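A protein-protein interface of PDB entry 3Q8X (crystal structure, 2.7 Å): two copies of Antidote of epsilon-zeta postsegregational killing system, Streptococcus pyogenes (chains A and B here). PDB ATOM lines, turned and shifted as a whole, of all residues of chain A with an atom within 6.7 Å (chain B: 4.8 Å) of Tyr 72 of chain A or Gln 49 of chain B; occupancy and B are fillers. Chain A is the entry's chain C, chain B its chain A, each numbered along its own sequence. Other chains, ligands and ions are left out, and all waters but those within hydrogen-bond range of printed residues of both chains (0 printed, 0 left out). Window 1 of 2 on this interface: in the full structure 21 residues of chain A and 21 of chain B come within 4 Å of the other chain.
Printed residues of chain B that touch a printed residue of chain A: Asn 45, Asn 48, Gln 49, Leu 52, Ala 53, Tyr 72 and Tyr 79. Hydrophobic or aromatic side chains of chain B within 4 Å of the printed part of chain A: Leu 52, Tyr 72 and Tyr 79. Along chain B the printed residues that touch a printed residue of chain A span positions 45 to 79. Hydrophobic or aromatic side chains of chain A within 4 Å of the printed part of chain B: Leu 52, Ala 53 and Tyr 72. Among the printed residues, no Asp or Glu carboxylate lies within 4 Å of a Lys or Arg side-chain nitrogen of the other chain.
Tyr 72 of chain A touches two residues of chain B. Gln 49 of chain B touches four residues of chain A. Of the printed residues of chain A, Tyr 72 of chain B touches Gln 49. Printed residues of chain B within 4 Å of Gln 49 of chain A: Gln 49, Leu 52 and Tyr 72. Of the printed residues of chain B, Asn 45 of chain A touches Leu 52 (3.1 Å) and Ala 53 (3.7 Å). Of the printed residues of chain B, Ala 68 of chain A touches Tyr 79. The nearest printed residue of chain A that does not touch Asn 45 of chain B is Gln 49 of chain A (5.4 Å).
O of Leu 52 of chain A is in hydrogen-bond range of ND2 of Asn 45 of chain B (3.2 Å). The side-chain amide oxygen (OE1) of Gln 49 of chain B sits at hydrogen-bond distance from the side-chain hydroxyl (OH) of Tyr 72 of chain A (2.6 Å). O of Leu 52 of chain B lies within hydrogen-bond range of ND2 of Asn 45 of chain A (3.1 Å). OH of Tyr 72 of chain B lies within hydrogen-bond range of OE1 of Gln 49 of chain A, at 2.4 Å.
OD1 of Asn 45 of chain A touches CA of Ala 53 of chain B (3.7 Å). Leu 52 of chain B touches Asn 48 of chain A. Gln 49 of chain A touches Gln 49 of chain B. CD1 of Leu 52 of chain B touches N of Gln 49 of chain A (3.98 Å). Leu 52 of chain A touches Asn 48 of chain B. Leu 52 of chain A touches Gln 49 of chain B (CD2 to N, 3.8 Å). Asn 45 of chain B touches Ala 53 of chain A (OD1 to CA, 3.3 Å). CB of Ala 53 of chain A touches NE2 of Gln 49 of chain B, at 3.6 Å. Ala 68 of chain A touches Tyr 79 of chain B (O to CE1, 3.3 Å). Tyr 72 of chain A touches Tyr 79 of chain B.
Asn 45 of chain A touches Leu 52 of chain B, and with the chains exchanged Leu 52 of chain A touches Asn 45 of chain B. Asn 45 of chain A touches Ala 53 of chain B, and with the chains exchanged Ala 53 of chain A touches Asn 45 of chain B. Gln 49 of chain A touches Leu 52 of chain B, and with the chains exchanged Leu 52 of chain A touches Gln 49 of chain B. Gln 49 of chain A touches Tyr 72 of chain B, and with the chains exchanged Tyr 72 of chain A touches Gln 49 of chain B. Positions printed for both chains: 45, 46, 48, 49, 50, 51, 52, 53, 72 and 76. Of the 14 pairs that touch across the chains among the printed residues, 11 have their exchanged pair printed and touching as well.
OD1 of Asn 45 of chain B lies within hydrogen-bond range of NE2 of Gln 49 of chain B. The side-chain amide oxygen (OD1) of Asn 45 of chain A lies within hydrogen-bond range of the side-chain amide nitrogen (NE2) of Gln 49 of chain A (2.9 Å).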
ATOM      1  N   LEU A  17      -5.642  18.733 -10.354  1.00  0.00           N
ATOM      2  CA  LEU A  17      -6.603  19.615  -9.703  1.00  0.00           C
ATOM      3  C   LEU A  17      -8.048  19.292 -10.062  1.00  0.00           C
ATOM      4  O   LEU A  17      -8.897  19.192  -9.165  1.00  0.00           O
ATOM      5  CB  LEU A  17      -6.304  21.075 -10.015  1.00  0.00           C
ATOM      6  CG  LEU A  17      -7.177  22.123  -9.329  1.00  0.00           C
ATOM      7  CD1 LEU A  17      -7.102  22.045  -7.804  1.00  0.00           C
ATOM      8  CD2 LEU A  17      -6.752  23.477  -9.805  1.00  0.00           C
ATOM      9  N   ASN A  45     -26.327  19.340  -9.996  1.00  0.00           N
ATOM     10  CA  ASN A  45     -26.148  20.348 -11.038  1.00  0.00           C
ATOM     11  C   ASN A  45     -24.672  20.760 -11.171  1.00  0.00           C
ATOM     12  O   ASN A  45     -24.163  20.963 -12.281  1.00  0.00           O
ATOM     13  CB  ASN A  45     -27.030  21.558 -10.765  1.00  0.00           C
ATOM     14  CG  ASN A  45     -27.069  22.531 -11.935  1.00  0.00           C
ATOM     15  OD1 ASN A  45     -26.254  23.442 -12.022  1.00  0.00           O
ATOM     16  ND2 ASN A  45     -28.038  22.356 -12.823  1.00  0.00           N
ATOM     17  N   LEU A  46     -23.985  20.862 -10.036  1.00  0.00           N
ATOM     18  CA  LEU A  46     -22.560  21.103 -10.041  1.00  0.00           C
ATOM     19  C   LEU A  46     -21.842  19.994 -10.788  1.00  0.00           C
ATOM     20  O   LEU A  46     -21.150  20.262 -11.755  1.00  0.00           O
ATOM     21  CB  LEU A  46     -22.029  21.213  -8.615  1.00  0.00           C
ATOM     22  CG  LEU A  46     -20.601  21.727  -8.425  1.00  0.00           C
ATOM     23  CD1 LEU A  46     -20.312  22.935  -9.299  1.00  0.00           C
ATOM     24  CD2 LEU A  46     -20.396  22.071  -6.965  1.00  0.00           C
ATOM     25  N   ASN A  48     -22.760  17.922 -12.979  1.00  0.00           N
ATOM     26  CA  ASN A  48     -23.020  17.947 -14.413  1.00  0.00           C
ATOM     27  C   ASN A  48     -22.235  19.020 -15.167  1.00  0.00           C
ATOM     28  O   ASN A  48     -21.788  18.796 -16.299  1.00  0.00           O
ATOM     29  CB  ASN A  48     -24.511  18.067 -14.676  1.00  0.00           C
ATOM     30  CG  ASN A  48     -25.238  16.794 -14.372  1.00  0.00           C
ATOM     31  OD1 ASN A  48     -24.652  15.718 -14.427  1.00  0.00           O
ATOM     32  ND2 ASN A  48     -26.520  16.900 -14.050  1.00  0.00           N
ATOM     33  N   GLN A  49     -22.058  20.175 -14.530  1.00  0.00           N
ATOM     34  CA  GLN A  49     -21.239  21.235 -15.096  1.00  0.00           C
ATOM     35  C   GLN A  49     -19.799  20.779 -15.213  1.00  0.00           C
ATOM     36  O   GLN A  49     -19.162  20.997 -16.235  1.00  0.00           O
ATOM     37  CB  GLN A  49     -21.321  22.482 -14.237  1.00  0.00           C
ATOM     38  CG  GLN A  49     -22.666  23.126 -14.298  1.00  0.00           C
ATOM     39  CD  GLN A  49     -22.758  24.302 -13.402  1.00  0.00           C
ATOM     40  OE1 GLN A  49     -22.261  25.378 -13.722  1.00  0.00           O
ATOM     41  NE2 GLN A  49     -23.394  24.117 -12.263  1.00  0.00           N
ATOM     42  N   LEU A  50     -19.297  20.135 -14.163  1.00  0.00           N
ATOM     43  CA  LEU A  50     -17.930  19.631 -14.164  1.00  0.00           C
ATOM     44  C   LEU A  50     -17.736  18.526 -15.203  1.00  0.00           C
ATOM     45  O   LEU A  50     -16.727  18.511 -15.900  1.00  0.00           O
ATOM     46  CB  LEU A  50     -17.516  19.171 -12.764  1.00  0.00           C
ATOM     47  CG  LEU A  50     -17.678  20.215 -11.651  1.00  0.00           C
ATOM     48  CD1 LEU A  50     -17.072  19.709 -10.352  1.00  0.00           C
ATOM     49  CD2 LEU A  50     -17.053  21.551 -12.026  1.00  0.00           C
ATOM     50  N   LYS A  51     -18.718  17.629 -15.324  1.00  0.00           N
ATOM     51  CA  LYS A  51     -18.712  16.613 -16.372  1.00  0.00           C
ATOM     52  C   LYS A  51     -18.526  17.307 -17.702  1.00  0.00           C
ATOM     53  O   LYS A  51     -17.884  16.778 -18.623  1.00  0.00           O
ATOM     54  CB  LYS A  51     -20.026  15.823 -16.387  1.00  0.00           C
ATOM     55  CG  LYS A  51     -20.048  14.663 -15.417  1.00  0.00           C
ATOM     56  CD  LYS A  51     -21.384  13.961 -15.406  1.00  0.00           C
ATOM     57  CE  LYS A  51     -21.396  12.827 -14.380  1.00  0.00           C
ATOM     58  NZ  LYS A  51     -20.456  11.727 -14.723  1.00  0.00           N
ATOM     59  N   LEU A  52     -19.082  18.512 -17.782  1.00  0.00           N
ATOM     60  CA  LEU A  52     -19.042  19.301 -18.993  1.00  0.00           C
ATOM     61  C   LEU A  52     -17.676  19.959 -19.190  1.00  0.00           C
ATOM     62  O   LEU A  52     -17.114  19.895 -20.277  1.00  0.00           O
ATOM     63  CB  LEU A  52     -20.155  20.339 -18.951  1.00  0.00           C
ATOM     64  CG  LEU A  52     -20.811  20.737 -20.266  1.00  0.00           C
ATOM     65  CD1 LEU A  52     -21.585  19.561 -20.866  1.00  0.00           C
ATOM     66  CD2 LEU A  52     -21.722  21.927 -20.002  1.00  0.00           C
ATOM     67  N   ALA A  53     -17.143  20.566 -18.131  1.00  0.00           N
ATOM     68  CA  ALA A  53     -15.849  21.245 -18.189  1.00  0.00           C
ATOM     69  C   ALA A  53     -14.704  20.266 -18.414  1.00  0.00           C
ATOM     70  O   ALA A  53     -13.772  20.555 -19.168  1.00  0.00           O
ATOM     71  CB  ALA A  53     -15.620  22.060 -16.950  1.00  0.00           C
ATOM     72  N   LYS A  54     -14.805  19.095 -17.788  1.00  0.00           N
ATOM     73  CA  LYS A  54     -13.803  18.037 -17.915  1.00  0.00           C
ATOM     74  C   LYS A  54     -13.789  17.373 -19.302  1.00  0.00           C
ATOM     75  O   LYS A  54     -12.904  16.575 -19.606  1.00  0.00           O
ATOM     76  CB  LYS A  54     -14.035  16.981 -16.828  1.00  0.00           C
ATOM     77  CG  LYS A  54     -12.776  16.210 -16.386  1.00  0.00           C
ATOM     78  CD  LYS A  54     -13.064  15.276 -15.208  1.00  0.00           C
ATOM     79  CE  LYS A  54     -14.173  14.284 -15.562  1.00  0.00           C
ATOM     80  NZ  LYS A  54     -14.267  13.142 -14.605  1.00  0.00           N
ATOM     81  N   GLN A  67      -4.313  28.703 -18.888  1.00  0.00           N
ATOM     82  CA  GLN A  67      -4.273  29.445 -17.624  1.00  0.00           C
ATOM     83  C   GLN A  67      -5.683  29.785 -17.160  1.00  0.00           C
ATOM     84  O   GLN A  67      -6.005  29.662 -15.978  1.00  0.00           O
ATOM     85  CB  GLN A  67      -3.399  30.694 -17.746  1.00  0.00           C
ATOM     86  CG  GLN A  67      -1.912  30.362 -17.754  1.00  0.00           C
ATOM     87  CD  GLN A  67      -1.043  31.465 -18.331  1.00  0.00           C
ATOM     88  OE1 GLN A  67      -1.531  32.381 -18.995  1.00  0.00           O
ATOM     89  NE2 GLN A  67       0.263  31.372 -18.089  1.00  0.00           N
ATOM     90  N   ALA A  68      -6.523  30.187 -18.113  1.00  0.00           N
ATOM     91  CA  ALA A  68      -7.941  30.395 -17.864  1.00  0.00           C
ATOM     92  C   ALA A  68      -8.556  29.135 -17.273  1.00  0.00           C
ATOM     93  O   ALA A  68      -9.275  29.219 -16.279  1.00  0.00           O
ATOM     94  CB  ALA A  68      -8.646  30.789 -19.137  1.00  0.00           C
ATOM     95  N   VAL A  69      -8.255  27.975 -17.864  1.00  0.00           N
ATOM     96  CA  VAL A  69      -8.795  26.694 -17.384  1.00  0.00           C
ATOM     97  C   VAL A  69      -8.238  26.322 -16.010  1.00  0.00           C
ATOM     98  O   VAL A  69      -8.948  25.764 -15.163  1.00  0.00           O
ATOM     99  CB  VAL A  69      -8.544  25.541 -18.368  1.00  0.00           C
ATOM    100  CG1 VAL A  69      -9.091  24.252 -17.818  1.00  0.00           C
ATOM    101  CG2 VAL A  69      -9.190  25.830 -19.701  1.00  0.00           C
ATOM    102  N   HIS A  70      -6.968  26.625 -15.791  1.00  0.00           N
ATOM    103  CA  HIS A  70      -6.398  26.538 -14.467  1.00  0.00           C
ATOM    104  C   HIS A  70      -7.250  27.378 -13.516  1.00  0.00           C
ATOM    105  O   HIS A  70      -7.633  26.905 -12.440  1.00  0.00           O
ATOM    106  CB  HIS A  70      -4.970  27.061 -14.484  1.00  0.00           C
ATOM    107  CG  HIS A  70      -4.121  26.563 -13.357  1.00  0.00           C
ATOM    108  ND1 HIS A  70      -2.745  26.667 -13.367  1.00  0.00           N
ATOM    109  CD2 HIS A  70      -4.444  25.955 -12.191  1.00  0.00           C
ATOM    110  CE1 HIS A  70      -2.259  26.153 -12.252  1.00  0.00           C
ATOM    111  NE2 HIS A  70      -3.269  25.712 -11.522  1.00  0.00           N
ATOM    112  N   GLU A  71      -7.571  28.610 -13.911  1.00  0.00           N
ATOM    113  CA  GLU A  71      -8.329  29.499 -13.032  1.00  0.00           C
ATOM    114  C   GLU A  71      -9.746  28.989 -12.739  1.00  0.00           C
ATOM    115  O   GLU A  71     -10.265  29.197 -11.644  1.00  0.00           O
ATOM    116  CB  GLU A  71      -8.346  30.942 -13.561  1.00  0.00           C
ATOM    117  CG  GLU A  71      -9.119  31.943 -12.687  1.00  0.00           C
ATOM    118  CD  GLU A  71      -8.707  31.918 -11.211  1.00  0.00           C
ATOM    119  OE1 GLU A  71      -7.492  31.813 -10.938  1.00  0.00           O
ATOM    120  OE2 GLU A  71      -9.598  32.012 -10.327  1.00  0.00           O
ATOM    121  N   TYR A  72     -10.352  28.318 -13.714  1.00  0.00           N
ATOM    122  CA  TYR A  72     -11.682  27.762 -13.553  1.00  0.00           C
ATOM    123  C   TYR A  72     -11.706  26.749 -12.415  1.00  0.00           C
ATOM    124  O   TYR A  72     -12.532  26.829 -11.500  1.00  0.00           O
ATOM    125  CB  TYR A  72     -12.136  27.094 -14.855  1.00  0.00           C
ATOM    126  CG  TYR A  72     -13.388  26.239 -14.709  1.00  0.00           C
ATOM    127  CD1 TYR A  72     -14.667  26.808 -14.794  1.00  0.00           C
ATOM    128  CD2 TYR A  72     -13.290  24.870 -14.476  1.00  0.00           C
ATOM    129  CE1 TYR A  72     -15.815  26.033 -14.655  1.00  0.00           C
ATOM    130  CE2 TYR A  72     -14.417  24.092 -14.324  1.00  0.00           C
ATOM    131  CZ  TYR A  72     -15.682  24.671 -14.421  1.00  0.00           C
ATOM    132  OH  TYR A  72     -16.800  23.871 -14.274  1.00  0.00           O
ATOM    133  N   TRP A  73     -10.802  25.781 -12.490  1.00  0.00           N
ATOM    134  CA  TRP A  73     -10.751  24.715 -11.510  1.00  0.00           C
ATOM    135  C   TRP A  73     -10.300  25.202 -10.125  1.00  0.00           C
ATOM    136  O   TRP A  73     -10.496  24.495  -9.138  1.00  0.00           O
ATOM    137  CB  TRP A  73      -9.866  23.580 -12.016  1.00  0.00           C
ATOM    138  CG  TRP A  73     -10.444  22.853 -13.190  1.00  0.00           C
ATOM    139  CD1 TRP A  73     -10.073  22.979 -14.491  1.00  0.00           C
ATOM    140  CD2 TRP A  73     -11.499  21.883 -13.165  1.00  0.00           C
ATOM    141  NE1 TRP A  73     -10.827  22.145 -15.286  1.00  0.00           N
ATOM    142  CE2 TRP A  73     -11.713  21.465 -14.495  1.00  0.00           C
ATOM    143  CE3 TRP A  73     -12.288  21.333 -12.147  1.00  0.00           C
ATOM    144  CZ2 TRP A  73     -12.683  20.517 -14.836  1.00  0.00           C
ATOM    145  CZ3 TRP A  73     -13.245  20.391 -12.481  1.00  0.00           C
ATOM    146  CH2 TRP A  73     -13.439  19.994 -13.820  1.00  0.00           C
ATOM    147  N   ARG A  74      -9.700  26.391 -10.045  1.00  0.00           N
ATOM    148  CA  ARG A  74      -9.481  27.020  -8.742  1.00  0.00           C
ATOM    149  C   ARG A  74     -10.796  27.533  -8.187  1.00  0.00           C
ATOM    150  O   ARG A  74     -11.048  27.403  -6.996  1.00  0.00           O
ATOM    151  CB  ARG A  74      -8.473  28.166  -8.805  1.00  0.00           C
ATOM    152  CG  ARG A  74      -7.029  27.742  -8.687  1.00  0.00           C
ATOM    153  CD  ARG A  74      -6.133  28.963  -8.558  1.00  0.00           C
ATOM    154  NE  ARG A  74      -4.863  28.770  -9.257  1.00  0.00           N
ATOM    155  CZ  ARG A  74      -4.598  29.217 -10.483  1.00  0.00           C
ATOM    156  NH1 ARG A  74      -5.509  29.906 -11.161  1.00  0.00           N
ATOM    157  NH2 ARG A  74      -3.415  28.985 -11.030  1.00  0.00           N
ATOM    158  N   SER A  75     -11.623  28.121  -9.051  1.00  0.00           N
ATOM    159  CA  SER A  75     -12.980  28.520  -8.677  1.00  0.00           C
ATOM    160  C   SER A  75     -13.800  27.346  -8.170  1.00  0.00           C
ATOM    161  O   SER A  75     -14.336  27.397  -7.064  1.00  0.00           O
ATOM    162  CB  SER A  75     -13.709  29.188  -9.832  1.00  0.00           C
ATOM    163  OG  SER A  75     -13.593  30.583  -9.718  1.00  0.00           O
ATOM    164  N   MET A  76     -13.891  26.291  -8.974  1.00  0.00           N
ATOM    165  CA  MET A  76     -14.650  25.120  -8.567  1.00  0.00           C
ATOM    166  C   MET A  76     -14.103  24.504  -7.280  1.00  0.00           C
ATOM    167  O   MET A  76     -14.867  24.072  -6.420  1.00  0.00           O
ATOM    168  CB  MET A  76     -14.728  24.089  -9.684  1.00  0.00           C
ATOM    169  CG  MET A  76     -15.572  24.543 -10.856  1.00  0.00           C
ATOM    170  SD  MET A  76     -17.022  25.441 -10.307  1.00  0.00           S
ATOM    171  CE  MET A  76     -18.148  25.226 -11.677  1.00  0.00           C
ATOM    172  N   ASN A  77     -12.783  24.492  -7.138  1.00  0.00           N
ATOM    173  CA  ASN A  77     -12.180  24.081  -5.887  1.00  0.00           C
ATOM    174  C   ASN A  77     -12.723  24.905  -4.727  1.00  0.00           C
ATOM    175  O   ASN A  77     -13.272  24.353  -3.777  1.00  0.00           O
ATOM    176  CB  ASN A  77     -10.659  24.200  -5.960  1.00  0.00           C
ATOM    177  CG  ASN A  77      -9.965  23.601  -4.751  1.00  0.00           C
ATOM    178  OD1 ASN A  77     -10.315  22.514  -4.283  1.00  0.00           O
ATOM    179  ND2 ASN A  77      -8.965  24.307  -4.247  1.00  0.00           N
ATOM    180  N   ARG A  78     -12.584  26.224  -4.817  1.00  0.00           N
ATOM    181  CA  ARG A  78     -13.066  27.112  -3.772  1.00  0.00           C
ATOM    182  C   ARG A  78     -14.554  26.911  -3.528  1.00  0.00           C
ATOM    183  O   ARG A  78     -15.002  26.813  -2.384  1.00  0.00           O
ATOM    184  CB  ARG A  78     -12.798  28.568  -4.137  1.00  0.00           C
ATOM    185  CG  ARG A  78     -11.414  29.058  -3.779  1.00  0.00           C
ATOM    186  CD  ARG A  78     -11.325  30.560  -3.967  1.00  0.00           C
ATOM    187  NE  ARG A  78     -11.449  30.941  -5.373  1.00  0.00           N
ATOM    188  CZ  ARG A  78     -10.438  30.967  -6.241  1.00  0.00           C
ATOM    189  NH1 ARG A  78      -9.205  30.633  -5.855  1.00  0.00           N
ATOM    190  NH2 ARG A  78     -10.660  31.330  -7.498  1.00  0.00           N
ATOM    191  N   ASN B  45     -18.153  26.271 -23.943  1.00  0.00           N
ATOM    192  CA  ASN B  45     -18.250  25.383 -22.790  1.00  0.00           C
ATOM    193  C   ASN B  45     -18.817  26.136 -21.599  1.00  0.00           C
ATOM    194  O   ASN B  45     -19.761  25.674 -20.960  1.00  0.00           O
ATOM    195  CB  ASN B  45     -16.899  24.780 -22.432  1.00  0.00           C
ATOM    196  CG  ASN B  45     -17.028  23.492 -21.622  1.00  0.00           C
ATOM    197  OD1 ASN B  45     -16.825  23.491 -20.414  1.00  0.00           O
ATOM    198  ND2 ASN B  45     -17.366  22.391 -22.288  1.00  0.00           N
ATOM    199  N   LEU B  46     -18.268  27.318 -21.329  1.00  0.00           N
ATOM    200  CA  LEU B  46     -18.744  28.145 -20.229  1.00  0.00           C
ATOM    201  C   LEU B  46     -20.191  28.517 -20.426  1.00  0.00           C
ATOM    202  O   LEU B  46     -20.982  28.411 -19.482  1.00  0.00           O
ATOM    203  CB  LEU B  46     -17.900  29.405 -20.062  1.00  0.00           C
ATOM    204  CG  LEU B  46     -18.408  30.464 -19.083  1.00  0.00           C
ATOM    205  CD1 LEU B  46     -18.476  29.905 -17.668  1.00  0.00           C
ATOM    206  CD2 LEU B  46     -17.544  31.710 -19.141  1.00  0.00           C
ATOM    207  N   LEU B  47     -20.555  28.940 -21.634  1.00  0.00           N
ATOM    208  CA  LEU B  47     -21.970  29.241 -21.904  1.00  0.00           C
ATOM    209  C   LEU B  47     -22.885  28.044 -21.576  1.00  0.00           C
ATOM    210  O   LEU B  47     -23.883  28.194 -20.859  1.00  0.00           O
ATOM    211  CB  LEU B  47     -22.189  29.703 -23.346  1.00  0.00           C
ATOM    212  CG  LEU B  47     -23.585  30.227 -23.708  1.00  0.00           C
ATOM    213  CD1 LEU B  47     -23.796  31.579 -23.087  1.00  0.00           C
ATOM    214  CD2 LEU B  47     -23.760  30.303 -25.216  1.00  0.00           C
ATOM    215  N   ASN B  48     -22.538  26.861 -22.082  1.00  0.00           N
ATOM    216  CA  ASN B  48     -23.317  25.678 -21.773  1.00  0.00           C
ATOM    217  C   ASN B  48     -23.429  25.399 -20.270  1.00  0.00           C
ATOM    218  O   ASN B  48     -24.471  24.960 -19.789  1.00  0.00           O
ATOM    219  CB  ASN B  48     -22.788  24.462 -22.530  1.00  0.00           C
ATOM    220  CG  ASN B  48     -22.911  24.616 -24.034  1.00  0.00           C
ATOM    221  OD1 ASN B  48     -23.776  25.341 -24.529  1.00  0.00           O
ATOM    222  ND2 ASN B  48     -22.038  23.933 -24.773  1.00  0.00           N
ATOM    223  N   GLN B  49     -22.365  25.676 -19.524  1.00  0.00           N
ATOM    224  CA  GLN B  49     -22.407  25.475 -18.084  1.00  0.00           C
ATOM    225  C   GLN B  49     -23.410  26.424 -17.448  1.00  0.00           C
ATOM    226  O   GLN B  49     -24.206  26.013 -16.612  1.00  0.00           O
ATOM    227  CB  GLN B  49     -21.031  25.658 -17.467  1.00  0.00           C
ATOM    228  CG  GLN B  49     -20.144  24.430 -17.554  1.00  0.00           C
ATOM    229  CD  GLN B  49     -18.737  24.729 -17.089  1.00  0.00           C
ATOM    230  OE1 GLN B  49     -18.505  25.004 -15.912  1.00  0.00           O
ATOM    231  NE2 GLN B  49     -17.793  24.707 -18.015  1.00  0.00           N
ATOM    232  N   LEU B  50     -23.380  27.683 -17.869  1.00  0.00           N
ATOM    233  CA  LEU B  50     -24.356  28.667 -17.415  1.00  0.00           C
ATOM    234  C   LEU B  50     -25.793  28.272 -17.755  1.00  0.00           C
ATOM    235  O   LEU B  50     -26.717  28.552 -16.981  1.00  0.00           O
ATOM    236  CB  LEU B  50     -24.035  30.047 -17.977  1.00  0.00           C
ATOM    237  CG  LEU B  50     -22.652  30.597 -17.598  1.00  0.00           C
ATOM    238  CD1 LEU B  50     -22.547  32.073 -17.975  1.00  0.00           C
ATOM    239  CD2 LEU B  50     -22.333  30.399 -16.122  1.00  0.00           C
ATOM    240  N   LYS B  51     -25.982  27.602 -18.893  1.00  0.00           N
ATOM    241  CA  LYS B  51     -27.319  27.151 -19.286  1.00  0.00           C
ATOM    242  C   LYS B  51     -27.878  26.143 -18.275  1.00  0.00           C
ATOM    243  O   LYS B  51     -29.019  26.293 -17.818  1.00  0.00           O
ATOM    244  CB  LYS B  51     -27.326  26.586 -20.710  1.00  0.00           C
ATOM    245  CG  LYS B  51     -27.424  27.641 -21.814  1.00  0.00           C
ATOM    246  CD  LYS B  51     -27.416  26.992 -23.206  1.00  0.00           C
ATOM    247  CE  LYS B  51     -27.201  28.005 -24.338  1.00  0.00           C
ATOM    248  NZ  LYS B  51     -28.385  28.876 -24.565  1.00  0.00           N
ATOM    249  N   LEU B  52     -27.074  25.139 -17.914  1.00  0.00           N
ATOM    250  CA  LEU B  52     -27.457  24.175 -16.883  1.00  0.00           C
ATOM    251  C   LEU B  52     -27.808  24.865 -15.565  1.00  0.00           C
ATOM    252  O   LEU B  52     -28.794  24.519 -14.923  1.00  0.00           O
ATOM    253  CB  LEU B  52     -26.344  23.158 -16.628  1.00  0.00           C
ATOM    254  CG  LEU B  52     -25.936  22.162 -17.711  1.00  0.00           C
ATOM    255  CD1 LEU B  52     -24.746  21.335 -17.229  1.00  0.00           C
ATOM    256  CD2 LEU B  52     -27.096  21.251 -18.110  1.00  0.00           C
ATOM    257  N   ALA B  53     -26.992  25.836 -15.167  1.00  0.00           N
ATOM    258  CA  ALA B  53     -27.183  26.539 -13.900  1.00  0.00           C
ATOM    259  C   ALA B  53     -28.576  27.191 -13.801  1.00  0.00           C
ATOM    260  O   ALA B  53     -29.272  27.051 -12.783  1.00  0.00           O
ATOM    261  CB  ALA B  53     -26.085  27.564 -13.702  1.00  0.00           C
ATOM    262  N   TYR B  72     -22.179  30.994  -6.378  1.00  0.00           N
ATOM    263  CA  TYR B  72     -21.882  30.473  -7.708  1.00  0.00           C
ATOM    264  C   TYR B  72     -21.804  31.604  -8.734  1.00  0.00           C
ATOM    265  O   TYR B  72     -20.826  31.707  -9.461  1.00  0.00           O
ATOM    266  CB  TYR B  72     -22.916  29.438  -8.154  1.00  0.00           C
ATOM    267  CG  TYR B  72     -22.725  28.995  -9.581  1.00  0.00           C
ATOM    268  CD1 TYR B  72     -21.780  28.026  -9.904  1.00  0.00           C
ATOM    269  CD2 TYR B  72     -23.472  29.563 -10.613  1.00  0.00           C
ATOM    270  CE1 TYR B  72     -21.586  27.625 -11.225  1.00  0.00           C
ATOM    271  CE2 TYR B  72     -23.303  29.166 -11.931  1.00  0.00           C
ATOM    272  CZ  TYR B  72     -22.356  28.198 -12.238  1.00  0.00           C
ATOM    273  OH  TYR B  72     -22.170  27.802 -13.549  1.00  0.00           O
ATOM    274  N   MET B  76     -18.802  32.974 -11.202  1.00  0.00           N
ATOM    275  CA  MET B  76     -18.812  33.037 -12.664  1.00  0.00           C
ATOM    276  C   MET B  76     -18.649  34.469 -13.140  1.00  0.00           C
ATOM    277  O   MET B  76     -17.955  34.709 -14.114  1.00  0.00           O
ATOM    278  CB  MET B  76     -20.050  32.385 -13.284  1.00  0.00           C
ATOM    279  CG  MET B  76     -20.109  30.883 -13.126  1.00  0.00           C
ATOM    280  SD  MET B  76     -18.568  30.068 -13.579  1.00  0.00           S
ATOM    281  CE  MET B  76     -19.182  28.445 -14.033  1.00  0.00           C
ATOM    282  N   TYR B  79     -14.975  35.020 -12.935  1.00  0.00           N
ATOM    283  CA  TYR B  79     -14.306  34.178 -13.921  1.00  0.00           C
ATOM    284  C   TYR B  79     -14.553  34.594 -15.371  1.00  0.00           C
ATOM    285  O   TYR B  79     -13.613  34.612 -16.176  1.00  0.00           O
ATOM    286  CB  TYR B  79     -14.707  32.715 -13.710  1.00  0.00           C
ATOM    287  CG  TYR B  79     -14.139  31.773 -14.735  1.00  0.00           C
ATOM    288  CD1 TYR B  79     -12.767  31.523 -14.790  1.00  0.00           C
ATOM    289  CD2 TYR B  79     -14.968  31.139 -15.651  1.00  0.00           C
ATOM    290  CE1 TYR B  79     -12.237  30.666 -15.726  1.00  0.00           C
ATOM    291  CE2 TYR B  79     -14.450  30.274 -16.592  1.00  0.00           C
ATOM    292  CZ  TYR B  79     -13.083  30.043 -16.624  1.00  0.00           C
ATOM    293  OH  TYR B  79     -12.555  29.195 -17.562  1.00  0.00           O
